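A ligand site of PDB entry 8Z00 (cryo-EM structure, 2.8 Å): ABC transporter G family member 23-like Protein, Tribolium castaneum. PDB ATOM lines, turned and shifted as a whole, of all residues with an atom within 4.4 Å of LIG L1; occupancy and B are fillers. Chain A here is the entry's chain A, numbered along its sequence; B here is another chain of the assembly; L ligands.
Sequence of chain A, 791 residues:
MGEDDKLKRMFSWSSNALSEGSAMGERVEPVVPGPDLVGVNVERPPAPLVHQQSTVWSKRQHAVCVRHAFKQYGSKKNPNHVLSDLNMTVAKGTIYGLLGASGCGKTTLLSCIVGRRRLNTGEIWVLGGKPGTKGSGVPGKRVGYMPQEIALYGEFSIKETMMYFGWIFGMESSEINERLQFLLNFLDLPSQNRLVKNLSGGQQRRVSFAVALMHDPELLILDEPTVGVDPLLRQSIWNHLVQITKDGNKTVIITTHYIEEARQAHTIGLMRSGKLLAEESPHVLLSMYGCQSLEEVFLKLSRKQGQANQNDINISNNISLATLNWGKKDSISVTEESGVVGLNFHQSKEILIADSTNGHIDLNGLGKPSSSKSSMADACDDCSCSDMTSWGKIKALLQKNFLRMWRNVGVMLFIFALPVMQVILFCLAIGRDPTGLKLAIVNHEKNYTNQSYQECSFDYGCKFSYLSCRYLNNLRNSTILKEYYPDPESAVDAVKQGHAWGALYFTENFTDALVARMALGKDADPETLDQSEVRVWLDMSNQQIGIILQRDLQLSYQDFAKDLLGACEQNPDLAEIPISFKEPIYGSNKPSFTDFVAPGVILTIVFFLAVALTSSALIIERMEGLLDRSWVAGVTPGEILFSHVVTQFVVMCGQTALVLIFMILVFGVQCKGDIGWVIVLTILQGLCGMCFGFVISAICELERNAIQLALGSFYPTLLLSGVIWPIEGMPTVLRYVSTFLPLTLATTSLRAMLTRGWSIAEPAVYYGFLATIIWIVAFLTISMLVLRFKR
O6 of LIG L1 is in hydrogen-bond range of N of Glu 701, at 3.0 Å. An oxygen (O6) of LIG L1 sits at hydrogen-bond distance from the side-chain amide nitrogen of Asn 705, 2.5 Å away. The backbone NH (N) of Gly 410 of chain B lies within hydrogen-bond range of an oxygen (O6) of LG2 L2 (3.5 Å).
O16 of LG2 L2 lies close to O5 of LIG L1 (3.0 Å).
The side-chain hydroxyl (OG) of Ser 713 sits at hydrogen-bond distance from the backbone carbonyl oxygen (O) of Leu 709, 3.4 Å away. OG1 of Thr 717 sits at hydrogen-bond distance from O of Ser 713 (2.9 Å). O of Asn 705 is in hydrogen-bond range of SG of Cys 700 (3.7 Å). O of Leu 413 of chain B lies within hydrogen-bond range of N of Leu 418 of chain B (3.0 Å).
Phe 608 touches LIG L1 (CZ to C40, 3.9 Å). Phe 692 touches LIG L1 (CE2 to C38, 3.98 Å). Ile 699 touches LIG L1. Cys 700 touches LIG L1 (SG to C41, 3.9 Å). Leu 702 touches LIG L1. Gln 708 touches LIG L1. CA of Gly 712 touches C19 of LIG L1, 3.9 Å away. CB of Ser 713 touches C39 of LIG L1 (3.5 Å). Thr 717 touches LIG L1 (OG1 to C40, 3.4 Å). CG of Pro 742 touches C38 of LIG L1, at 3.9 Å. Leu 413 of chain B touches LIG L1. Phe 414 of chain B touches LIG L1 (CD1 to C20, 3.9 Å). CD1 of Leu 418 of chain B touches C18 of LIG L1 (3.9 Å). Met 421 of chain B touches LIG L1 (CE to C16, 3.4 Å). Hydrophobic or aromatic side chains within 4 Å of LIG L1: Phe 608, Phe 692, Ile 699, Pro 742, Leu 413 of chain B, Phe 414 of chain B, Leu 418 of chain B and Met 421 of chain B. Within 4 Å of LIG L1: Phe 608, Phe 692, Ile 699, Cys 700, Glu 701, Leu 702, Asn 705, Gln 708, Gly 712, Ser 713, Thr 717, Pro 742, Leu 413 of chain B, Phe 414 of chain B, Leu 418 of chain B and Met 421 of chain B.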
ATOM      1  N   PHE A 607      -9.128  -3.643  21.708  1.00  0.00           N
ATOM      2  CA  PHE A 607      -8.392  -2.910  20.685  1.00  0.00           C
ATOM      3  C   PHE A 607      -7.743  -3.860  19.683  1.00  0.00           C
ATOM      4  O   PHE A 607      -7.919  -3.706  18.467  1.00  0.00           O
ATOM      5  CB  PHE A 607      -7.334  -2.012  21.325  1.00  0.00           C
ATOM      6  CG  PHE A 607      -6.600  -1.125  20.354  1.00  0.00           C
ATOM      7  CD1 PHE A 607      -5.482  -1.591  19.678  1.00  0.00           C
ATOM      8  CD2 PHE A 607      -7.025   0.170  20.131  1.00  0.00           C
ATOM      9  CE1 PHE A 607      -4.814  -0.776  18.788  1.00  0.00           C
ATOM     10  CE2 PHE A 607      -6.349   0.989  19.239  1.00  0.00           C
ATOM     11  CZ  PHE A 607      -5.248   0.513  18.568  1.00  0.00           C
ATOM     12  N   PHE A 608      -7.001  -4.852  20.167  1.00  0.00           N
ATOM     13  CA  PHE A 608      -6.210  -5.700  19.285  1.00  0.00           C
ATOM     14  C   PHE A 608      -7.009  -6.808  18.631  1.00  0.00           C
ATOM     15  O   PHE A 608      -6.507  -7.431  17.689  1.00  0.00           O
ATOM     16  CB  PHE A 608      -5.026  -6.280  20.058  1.00  0.00           C
ATOM     17  CG  PHE A 608      -3.950  -5.280  20.384  1.00  0.00           C
ATOM     18  CD1 PHE A 608      -3.140  -4.773  19.375  1.00  0.00           C
ATOM     19  CD2 PHE A 608      -3.763  -4.834  21.679  1.00  0.00           C
ATOM     20  CE1 PHE A 608      -2.158  -3.851  19.672  1.00  0.00           C
ATOM     21  CE2 PHE A 608      -2.787  -3.904  21.974  1.00  0.00           C
ATOM     22  CZ  PHE A 608      -1.981  -3.412  20.960  1.00  0.00           C
ATOM     23  N   PHE A 692      -7.035   1.405  12.786  1.00  0.00           N
ATOM     24  CA  PHE A 692      -5.653   0.951  12.640  1.00  0.00           C
ATOM     25  C   PHE A 692      -5.546  -0.245  11.701  1.00  0.00           C
ATOM     26  O   PHE A 692      -4.557  -0.380  10.989  1.00  0.00           O
ATOM     27  CB  PHE A 692      -5.061   0.624  14.011  1.00  0.00           C
ATOM     28  CG  PHE A 692      -3.618   0.219  13.970  1.00  0.00           C
ATOM     29  CD1 PHE A 692      -2.712   0.915  13.178  1.00  0.00           C
ATOM     30  CD2 PHE A 692      -3.159  -0.849  14.720  1.00  0.00           C
ATOM     31  CE1 PHE A 692      -1.383   0.547  13.140  1.00  0.00           C
ATOM     32  CE2 PHE A 692      -1.832  -1.221  14.673  1.00  0.00           C
ATOM     33  CZ  PHE A 692      -0.934  -0.529  13.883  1.00  0.00           C
ATOM     34  N   ILE A 699      -1.786  -0.995   3.388  1.00  0.00           N
ATOM     35  CA  ILE A 699      -0.346  -1.038   3.191  1.00  0.00           C
ATOM     36  C   ILE A 699       0.128  -2.421   2.784  1.00  0.00           C
ATOM     37  O   ILE A 699       0.868  -2.562   1.811  1.00  0.00           O
ATOM     38  CB  ILE A 699       0.375  -0.557   4.473  1.00  0.00           C
ATOM     39  CG1 ILE A 699       0.260   0.962   4.620  1.00  0.00           C
ATOM     40  CG2 ILE A 699       1.830  -0.984   4.468  1.00  0.00           C
ATOM     41  CD1 ILE A 699       1.031   1.514   5.802  1.00  0.00           C
ATOM     42  N   CYS A 700      -0.297  -3.452   3.507  1.00  0.00           N
ATOM     43  CA  CYS A 700       0.187  -4.801   3.287  1.00  0.00           C
ATOM     44  C   CYS A 700      -0.589  -5.499   2.168  1.00  0.00           C
ATOM     45  O   CYS A 700      -1.734  -5.145   1.863  1.00  0.00           O
ATOM     46  CB  CYS A 700       0.099  -5.624   4.569  1.00  0.00           C
ATOM     47  SG  CYS A 700       1.266  -5.113   5.851  1.00  0.00           S
ATOM     48  N   GLU A 701      -0.070  -6.547   1.555  1.00  0.00           N
ATOM     49  CA  GLU A 701      -0.844  -7.316   0.550  1.00  0.00           C
ATOM     50  C   GLU A 701      -0.882  -8.793   0.903  1.00  0.00           C
ATOM     51  O   GLU A 701      -1.602  -9.505   0.241  1.00  0.00           O
ATOM     52  CB  GLU A 701      -0.236  -7.268  -0.837  1.00  0.00           C
ATOM     53  CG  GLU A 701      -0.650  -6.067  -1.662  1.00  0.00           C
ATOM     54  CD  GLU A 701      -0.160  -6.185  -3.092  1.00  0.00           C
ATOM     55  OE1 GLU A 701       0.501  -7.198  -3.388  1.00  0.00           O
ATOM     56  OE2 GLU A 701      -0.442  -5.278  -3.881  1.00  0.00           O
ATOM     57  N   LEU A 702      -0.111  -9.229   1.895  1.00  0.00           N
ATOM     58  CA  LEU A 702      -0.239 -10.614   2.327  1.00  0.00           C
ATOM     59  C   LEU A 702      -0.637 -10.658   3.791  1.00  0.00           C
ATOM     60  O   LEU A 702      -0.340  -9.735   4.560  1.00  0.00           O
ATOM     61  CB  LEU A 702       1.071 -11.391   2.114  1.00  0.00           C
ATOM     62  CG  LEU A 702       1.361 -11.896   0.704  1.00  0.00           C
ATOM     63  CD1 LEU A 702       2.831 -11.710   0.365  1.00  0.00           C
ATOM     64  CD2 LEU A 702       0.972 -13.358   0.572  1.00  0.00           C
ATOM     65  N   ASN A 705       2.338 -10.643   6.206  1.00  0.00           N
ATOM     66  CA  ASN A 705       2.934  -9.332   6.429  1.00  0.00           C
ATOM     67  C   ASN A 705       2.102  -8.484   7.378  1.00  0.00           C
ATOM     68  O   ASN A 705       2.662  -7.705   8.155  1.00  0.00           O
ATOM     69  CB  ASN A 705       3.106  -8.598   5.099  1.00  0.00           C
ATOM     70  CG  ASN A 705       4.196  -9.193   4.233  1.00  0.00           C
ATOM     71  OD1 ASN A 705       5.128  -9.821   4.737  1.00  0.00           O
ATOM     72  ND2 ASN A 705       4.075  -9.011   2.930  1.00  0.00           N
ATOM     73  N   GLN A 708       2.724  -9.619  11.133  1.00  0.00           N
ATOM     74  CA  GLN A 708       3.966  -9.103  11.692  1.00  0.00           C
ATOM     75  C   GLN A 708       3.865  -7.615  11.992  1.00  0.00           C
ATOM     76  O   GLN A 708       4.490  -7.130  12.949  1.00  0.00           O
ATOM     77  CB  GLN A 708       5.126  -9.382  10.748  1.00  0.00           C
ATOM     78  CG  GLN A 708       5.378 -10.859  10.500  1.00  0.00           C
ATOM     79  CD  GLN A 708       6.431 -11.109   9.446  1.00  0.00           C
ATOM     80  OE1 GLN A 708       7.560 -10.634   9.570  1.00  0.00           O
ATOM     81  NE2 GLN A 708       6.077 -11.858   8.415  1.00  0.00           N
ATOM     82  N   LEU A 709       3.102  -6.870  11.193  1.00  0.00           N
ATOM     83  CA  LEU A 709       2.911  -5.444  11.470  1.00  0.00           C
ATOM     84  C   LEU A 709       2.079  -5.229  12.726  1.00  0.00           C
ATOM     85  O   LEU A 709       2.352  -4.318  13.511  1.00  0.00           O
ATOM     86  CB  LEU A 709       2.267  -4.756  10.264  1.00  0.00           C
ATOM     87  CG  LEU A 709       3.140  -3.809   9.447  1.00  0.00           C
ATOM     88  CD1 LEU A 709       2.284  -2.952   8.543  1.00  0.00           C
ATOM     89  CD2 LEU A 709       3.991  -2.949  10.364  1.00  0.00           C
ATOM     90  N   GLY A 712       4.196  -6.423  15.695  1.00  0.00           N
ATOM     91  CA  GLY A 712       5.297  -5.496  15.881  1.00  0.00           C
ATOM     92  C   GLY A 712       4.931  -4.213  16.587  1.00  0.00           C
ATOM     93  O   GLY A 712       5.834  -3.519  17.063  1.00  0.00           O
ATOM     94  N   SER A 713       3.642  -3.894  16.665  1.00  0.00           N
ATOM     95  CA  SER A 713       3.169  -2.750  17.424  1.00  0.00           C
ATOM     96  C   SER A 713       2.425  -3.138  18.694  1.00  0.00           C
ATOM     97  O   SER A 713       2.249  -2.287  19.573  1.00  0.00           O
ATOM     98  CB  SER A 713       2.241  -1.870  16.565  1.00  0.00           C
ATOM     99  OG  SER A 713       1.076  -2.576  16.187  1.00  0.00           O
ATOM    100  N   THR A 717       3.748  -1.149  22.519  1.00  0.00           N
ATOM    101  CA  THR A 717       2.779  -0.262  23.150  1.00  0.00           C
ATOM    102  C   THR A 717       2.254  -0.828  24.455  1.00  0.00           C
ATOM    103  O   THR A 717       1.918  -0.069  25.379  1.00  0.00           O
ATOM    104  CB  THR A 717       1.624   0.037  22.202  1.00  0.00           C
ATOM    105  OG1 THR A 717       0.926  -1.176  21.901  1.00  0.00           O
ATOM    106  CG2 THR A 717       2.139   0.646  20.907  1.00  0.00           C
ATOM    107  N   PRO A 742      -1.658   5.374  21.745  1.00  0.00           N
ATOM    108  CA  PRO A 742      -3.134   5.252  21.658  1.00  0.00           C
ATOM    109  C   PRO A 742      -3.814   4.823  22.943  1.00  0.00           C
ATOM    110  O   PRO A 742      -4.911   5.307  23.233  1.00  0.00           O
ATOM    111  CB  PRO A 742      -3.318   4.208  20.544  1.00  0.00           C
ATOM    112  CG  PRO A 742      -2.088   4.323  19.721  1.00  0.00           C
ATOM    113  CD  PRO A 742      -0.984   4.619  20.684  1.00  0.00           C
ATOM    114  N   LEU A 743      -3.204   3.942  23.726  1.00  0.00           N
ATOM    115  CA  LEU A 743      -3.877   3.318  24.856  1.00  0.00           C
ATOM    116  C   LEU A 743      -3.442   3.863  26.218  1.00  0.00           C
ATOM    117  O   LEU A 743      -3.911   3.371  27.243  1.00  0.00           O
ATOM    118  CB  LEU A 743      -3.654   1.797  24.833  1.00  0.00           C
ATOM    119  CG  LEU A 743      -4.340   1.022  23.704  1.00  0.00           C
ATOM    120  CD1 LEU A 743      -3.348   0.689  22.608  1.00  0.00           C
ATOM    121  CD2 LEU A 743      -4.980  -0.243  24.248  1.00  0.00           C
ATOM    122  N   PHE A 779      -5.845   7.994  12.206  1.00  0.00           N
ATOM    123  CA  PHE A 779      -5.799   6.713  11.508  1.00  0.00           C
ATOM    124  C   PHE A 779      -6.601   6.743  10.216  1.00  0.00           C
ATOM    125  O   PHE A 779      -6.222   6.106   9.230  1.00  0.00           O
ATOM    126  CB  PHE A 779      -6.308   5.598  12.433  1.00  0.00           C
ATOM    127  CG  PHE A 779      -5.262   5.073  13.375  1.00  0.00           C
ATOM    128  CD1 PHE A 779      -3.945   4.958  12.973  1.00  0.00           C
ATOM    129  CD2 PHE A 779      -5.602   4.691  14.657  1.00  0.00           C
ATOM    130  CE1 PHE A 779      -2.981   4.474  13.840  1.00  0.00           C
ATOM    131  CE2 PHE A 779      -4.646   4.203  15.526  1.00  0.00           C
ATOM    132  CZ  PHE A 779      -3.335   4.095  15.123  1.00  0.00           C
ATOM    133  N   GLY B 410      12.651  -7.747   6.171  1.00  0.00           N
ATOM    134  CA  GLY B 410      11.553  -7.798   7.128  1.00  0.00           C
ATOM    135  C   GLY B 410      11.636  -8.997   8.046  1.00  0.00           C
ATOM    136  O   GLY B 410      11.277  -8.919   9.230  1.00  0.00           O
ATOM    137  N   LEU B 413      14.298  -8.308  10.673  1.00  0.00           N
ATOM    138  CA  LEU B 413      13.860  -7.365  11.693  1.00  0.00           C
ATOM    139  C   LEU B 413      12.927  -8.009  12.704  1.00  0.00           C
ATOM    140  O   LEU B 413      12.928  -7.609  13.878  1.00  0.00           O
ATOM    141  CB  LEU B 413      13.185  -6.162  11.036  1.00  0.00           C
ATOM    142  CG  LEU B 413      14.098  -5.099  10.422  1.00  0.00           C
ATOM    143  CD1 LEU B 413      13.275  -3.976   9.836  1.00  0.00           C
ATOM    144  CD2 LEU B 413      15.080  -4.578  11.450  1.00  0.00           C
ATOM    145  N   PHE B 414      12.112  -8.972  12.283  1.00  0.00           N
ATOM    146  CA  PHE B 414      11.118  -9.547  13.177  1.00  0.00           C
ATOM    147  C   PHE B 414      11.716 -10.521  14.187  1.00  0.00           C
ATOM    148  O   PHE B 414      11.227 -10.596  15.316  1.00  0.00           O
ATOM    149  CB  PHE B 414      10.027 -10.250  12.360  1.00  0.00           C
ATOM    150  CG  PHE B 414       8.846 -10.683  13.174  1.00  0.00           C
ATOM    151  CD1 PHE B 414       7.917  -9.750  13.619  1.00  0.00           C
ATOM    152  CD2 PHE B 414       8.654 -12.012  13.492  1.00  0.00           C
ATOM    153  CE1 PHE B 414       6.829 -10.150  14.370  1.00  0.00           C
ATOM    154  CE2 PHE B 414       7.566 -12.412  14.243  1.00  0.00           C
ATOM    155  CZ  PHE B 414       6.657 -11.480  14.676  1.00  0.00           C
ATOM    156  N   ALA B 417      15.527  -7.973  15.672  1.00  0.00           N
ATOM    157  CA  ALA B 417      15.395  -6.623  16.214  1.00  0.00           C
ATOM    158  C   ALA B 417      14.200  -6.479  17.137  1.00  0.00           C
ATOM    159  O   ALA B 417      14.248  -5.678  18.076  1.00  0.00           O
ATOM    160  CB  ALA B 417      15.298  -5.610  15.079  1.00  0.00           C
ATOM    161  N   LEU B 418      13.119  -7.226  16.887  1.00  0.00           N
ATOM    162  CA  LEU B 418      11.978  -7.208  17.787  1.00  0.00           C
ATOM    163  C   LEU B 418      12.318  -7.699  19.194  1.00  0.00           C
ATOM    164  O   LEU B 418      11.890  -7.049  20.160  1.00  0.00           O
ATOM    165  CB  LEU B 418      10.832  -8.023  17.176  1.00  0.00           C
ATOM    166  CG  LEU B 418       9.497  -8.017  17.915  1.00  0.00           C
ATOM    167  CD1 LEU B 418       8.537  -7.022  17.299  1.00  0.00           C
ATOM    168  CD2 LEU B 418       8.884  -9.413  17.917  1.00  0.00           C
ATOM    169  N   MET B 421      14.142  -4.869  21.146  1.00  0.00           N
ATOM    170  CA  MET B 421      13.293  -3.750  21.539  1.00  0.00           C
ATOM    171  C   MET B 421      12.488  -4.086  22.781  1.00  0.00           C
ATOM    172  O   MET B 421      12.312  -3.232  23.670  1.00  0.00           O
ATOM    173  CB  MET B 421      12.379  -3.353  20.387  1.00  0.00           C
ATOM    174  CG  MET B 421      11.878  -1.928  20.451  1.00  0.00           C
ATOM    175  SD  MET B 421      10.113  -1.791  20.117  1.00  0.00           S
ATOM    176  CE  MET B 421      10.029  -2.542  18.488  1.00  0.00           C
HETATM  177  C1  LIG L   1       9.241  -4.597  13.579  1.00  0.00           C
HETATM  178  C2  LIG L   1       8.893  -5.429  11.032  1.00  0.00           C
HETATM  179  C3  LIG L   1       7.388  -6.806   9.495  1.00  0.00           C
HETATM  180  C4  LIG L   1       7.144  -5.767   7.197  1.00  0.00           C
HETATM  181  C5  LIG L   1       5.644  -5.005   3.856  1.00  0.00           C
HETATM  182  C6  LIG L   1       5.940  -3.569   3.452  1.00  0.00           C
HETATM  183  C7  LIG L   1       5.088  -1.628   4.522  1.00  0.00           C
HETATM  184  C8  LIG L   1       6.623  -0.758   6.357  1.00  0.00           C
HETATM  185  C9  LIG L   1       6.070   1.369   7.641  1.00  0.00           C
HETATM  186  C10 LIG L   1      17.794  -1.422  13.305  1.00  0.00           C
HETATM  187  C11 LIG L   1      16.914  -0.560  14.236  1.00  0.00           C
HETATM  188  C12 LIG L   1      15.551  -0.162  13.589  1.00  0.00           C
HETATM  189  C13 LIG L   1      14.531  -1.322  13.595  1.00  0.00           C
HETATM  190  C14 LIG L   1      13.229  -0.997  14.386  1.00  0.00           C
HETATM  191  C15 LIG L   1      12.985  -2.005  15.541  1.00  0.00           C
HETATM  192  C16 LIG L   1      11.570  -2.663  15.463  1.00  0.00           C
HETATM  193  C17 LIG L   1      11.524  -3.808  14.423  1.00  0.00           C
HETATM  194  C18 LIG L   1      10.336  -4.759  14.673  1.00  0.00           C
HETATM  195  C19 LIG L   1       8.317  -5.847  13.494  1.00  0.00           C
HETATM  196  C20 LIG L   1       7.989  -6.215  12.027  1.00  0.00           C
HETATM  197  C21 LIG L   1       8.443  -5.669   9.564  1.00  0.00           C
HETATM  198  C22 LIG L   1       6.913  -7.036   8.038  1.00  0.00           C
HETATM  199  C23 LIG L   1       6.610  -5.945   5.764  1.00  0.00           C
HETATM  200  C24 LIG L   1       5.872  -1.983   5.804  1.00  0.00           C
HETATM  201  C25 LIG L   1       5.717   0.486   6.428  1.00  0.00           C
HETATM  202  C26 LIG L   1       5.129   1.364   8.575  1.00  0.00           C
HETATM  203  C27 LIG L   1       3.761   0.930   9.150  1.00  0.00           C
HETATM  204  C28 LIG L   1       3.411   1.676  10.457  1.00  0.00           C
HETATM  205  C29 LIG L   1       2.653   2.758  10.221  1.00  0.00           C
HETATM  206  C30 LIG L   1       1.863   4.002  10.697  1.00  0.00           C
HETATM  207  C31 LIG L   1       1.577   3.930  12.208  1.00  0.00           C
HETATM  208  C32 LIG L   1       1.884   5.060  12.843  1.00  0.00           C
HETATM  209  C33 LIG L   1       1.396   4.304  14.103  1.00  0.00           C
HETATM  210  C34 LIG L   1       2.230   4.633  15.351  1.00  0.00           C
HETATM  211  C35 LIG L   1       2.079   3.714  16.302  1.00  0.00           C
HETATM  212  C36 LIG L   1       1.460   2.416  16.853  1.00  0.00           C
HETATM  213  C37 LIG L   1      -0.059   2.514  16.803  1.00  0.00           C
HETATM  214  C38 LIG L   1      -0.798   1.555  17.325  1.00  0.00           C
HETATM  215  C39 LIG L   1      -0.129   0.331  17.957  1.00  0.00           C
HETATM  216  C40 LIG L   1      -0.890  -0.120  19.206  1.00  0.00           C
HETATM  217  C41 LIG L   1       4.246  -5.338   3.327  1.00  0.00           C
HETATM  218  C42 LIG L   1       3.360  -4.710  -1.203  1.00  0.00           C
HETATM  219  C43 LIG L   1       3.378  -3.241  -0.776  1.00  0.00           C
HETATM  220  N1  LIG L   1       4.716  -2.681  -0.996  1.00  0.00           N
HETATM  221  O1  LIG L   1       7.019  -6.850   5.134  1.00  0.00           O
HETATM  222  O2  LIG L   1       5.646  -5.067   5.234  1.00  0.00           O
HETATM  223  O3  LIG L   1       4.795  -2.834   3.824  1.00  0.00           O
HETATM  224  O4  LIG L   1       4.285  -5.084   1.941  1.00  0.00           O
HETATM  225  O5  LIG L   1       4.615  -7.035   0.268  1.00  0.00           O
HETATM  226  O6  LIG L   1       2.888  -7.229   1.646  1.00  0.00           O
HETATM  227  O7  LIG L   1       2.695  -5.451  -0.198  1.00  0.00           O
HETATM  228  P1  LIG L   1       3.623  -6.216   0.932  1.00  0.00           P
HETATM  229  C1  LG2 L   2       8.438 -12.679   2.578  1.00  0.00           C
HETATM  230  O1  LG2 L   2       8.206 -13.903   3.176  1.00  0.00           O
HETATM  231  C2  LG2 L   2       7.193 -12.175   1.855  1.00  0.00           C
HETATM  232  O2  LG2 L   2       6.700 -13.128   0.962  1.00  0.00           O
HETATM  233  C3  LG2 L   2       7.645 -10.944   1.082  1.00  0.00           C
HETATM  234  O3  LG2 L   2       6.586 -10.475   0.315  1.00  0.00           O
HETATM  235  C4  LG2 L   2       8.058  -9.936   2.137  1.00  0.00           C
HETATM  236  O4  LG2 L   2       8.513  -8.755   1.524  1.00  0.00           O
HETATM  237  C5  LG2 L   2       9.194 -10.568   2.930  1.00  0.00           C
HETATM  238  O5  LG2 L   2       8.741 -11.719   3.566  1.00  0.00           O
HETATM  239  C6  LG2 L   2       9.683  -9.580   4.002  1.00  0.00           C
HETATM  240  O6  LG2 L   2      10.788  -8.897   3.462  1.00  0.00           O
HETATM  241  C7  LG2 L   2      14.840 -21.971  10.783  1.00  0.00           C
HETATM  242  C8  LG2 L   2       3.949 -14.980  12.939  1.00  0.00           C
HETATM  243  O7  LG2 L   2       9.105  -4.377   3.805  1.00  0.00           O
HETATM  244  O8  LG2 L   2       9.373 -17.127  -7.484  1.00  0.00           O
HETATM  245  O9  LG2 L   2       5.523 -17.624  -1.150  1.00  0.00           O
HETATM  246  O10 LG2 L   2      10.207 -14.201  -2.745  1.00  0.00           O
HETATM  247  O11 LG2 L   2      10.440 -14.294   0.038  1.00  0.00           O
HETATM  248  O12 LG2 L   2      10.253  -4.667   1.223  1.00  0.00           O
HETATM  249  O13 LG2 L   2       5.307 -16.288  -5.117  1.00  0.00           O
HETATM  250  O14 LG2 L   2       8.533  -5.252  -0.933  1.00  0.00           O
HETATM  251  O15 LG2 L   2       6.017 -13.870  -7.380  1.00  0.00           O
HETATM  252  O16 LG2 L   2       7.351  -7.834  -0.689  1.00  0.00           O
HETATM  253  O17 LG2 L   2       7.990 -12.861  -5.398  1.00  0.00           O
HETATM  254  C9  LG2 L   2      14.034 -22.013   9.502  1.00  0.00           C
HETATM  255  C10 LG2 L   2       4.949 -14.096  12.187  1.00  0.00           C
HETATM  256  C11 LG2 L   2      14.942 -21.744   8.318  1.00  0.00           C
HETATM  257  C12 LG2 L   2       5.288 -14.735  10.851  1.00  0.00           C
HETATM  258  C13 LG2 L   2      14.098 -21.190   7.186  1.00  0.00           C
HETATM  259  C14 LG2 L   2       6.494 -15.653  11.027  1.00  0.00           C
HETATM  260  C15 LG2 L   2      14.743 -19.934   6.644  1.00  0.00           C
HETATM  261  C16 LG2 L   2       7.781 -14.849  10.869  1.00  0.00           C
HETATM  262  C17 LG2 L   2      13.946 -19.448   5.452  1.00  0.00           C
HETATM  263  C18 LG2 L   2       8.613 -15.490   9.756  1.00  0.00           C
HETATM  264  C19 LG2 L   2      12.814 -18.571   5.949  1.00  0.00           C
HETATM  265  C20 LG2 L   2       7.998 -15.113   8.405  1.00  0.00           C
HETATM  266  C21 LG2 L   2      12.479 -17.555   4.863  1.00  0.00           C
HETATM  267  C22 LG2 L   2       8.368 -16.176   7.364  1.00  0.00           C
HETATM  268  C23 LG2 L   2      10.997 -17.650   4.517  1.00  0.00           C
HETATM  269  C24 LG2 L   2       8.585 -15.491   6.011  1.00  0.00           C
HETATM  270  C25 LG2 L   2       9.660  -5.656   3.766  1.00  0.00           C
HETATM  271  C26 LG2 L   2       8.001 -16.867  -7.608  1.00  0.00           C
HETATM  272  C27 LG2 L   2       6.245 -17.024  -2.196  1.00  0.00           C
HETATM  273  C28 LG2 L   2      10.689 -16.590   3.447  1.00  0.00           C
HETATM  274  C29 LG2 L   2       8.666 -16.563   4.935  1.00  0.00           C
HETATM  275  C30 LG2 L   2       9.356 -14.482   3.712  1.00  0.00           C
HETATM  276  C31 LG2 L   2       8.404 -16.414   2.453  1.00  0.00           C
HETATM  277  O18 LG2 L   2       9.196 -16.403   1.305  1.00  0.00           O
HETATM  278  O19 LG2 L   2       7.885 -16.711  -0.529  1.00  0.00           O
HETATM  279  O20 LG2 L   2       7.922  -6.901   2.712  1.00  0.00           O
HETATM  280  O21 LG2 L   2       8.312 -16.458  -5.250  1.00  0.00           O
HETATM  281  O22 LG2 L   2       7.582 -14.969  -3.658  1.00  0.00           O
HETATM  282  C32 LG2 L   2       9.175  -6.357   2.497  1.00  0.00           C
HETATM  283  C33 LG2 L   2       7.354 -16.841  -6.206  1.00  0.00           C
HETATM  284  C34 LG2 L   2       7.235 -16.050  -1.559  1.00  0.00           C
HETATM  285  C35 LG2 L   2       9.152 -14.575  -1.911  1.00  0.00           C
HETATM  286  C36 LG2 L   2       8.620 -15.782   0.205  1.00  0.00           C
HETATM  287  C37 LG2 L   2       9.735 -15.249  -0.682  1.00  0.00           C
HETATM  288  C38 LG2 L   2       9.276 -16.010   3.655  1.00  0.00           C
HETATM  289  C39 LG2 L   2       9.049  -5.348   1.377  1.00  0.00           C
HETATM  290  C40 LG2 L   2       6.091 -15.949  -6.221  1.00  0.00           C
HETATM  291  C41 LG2 L   2       8.252 -15.585  -2.591  1.00  0.00           C
HETATM  292  C42 LG2 L   2       7.567  -7.738   1.665  1.00  0.00           C
HETATM  293  C43 LG2 L   2       8.354 -15.120  -4.831  1.00  0.00           C
HETATM  294  C44 LG2 L   2       8.762  -6.136   0.129  1.00  0.00           C
HETATM  295  C45 LG2 L   2       6.376 -14.447  -6.161  1.00  0.00           C
HETATM  296  C46 LG2 L   2       7.494  -6.938   0.357  1.00  0.00           C
HETATM  297  C47 LG2 L   2       7.836 -14.164  -5.887  1.00  0.00           C
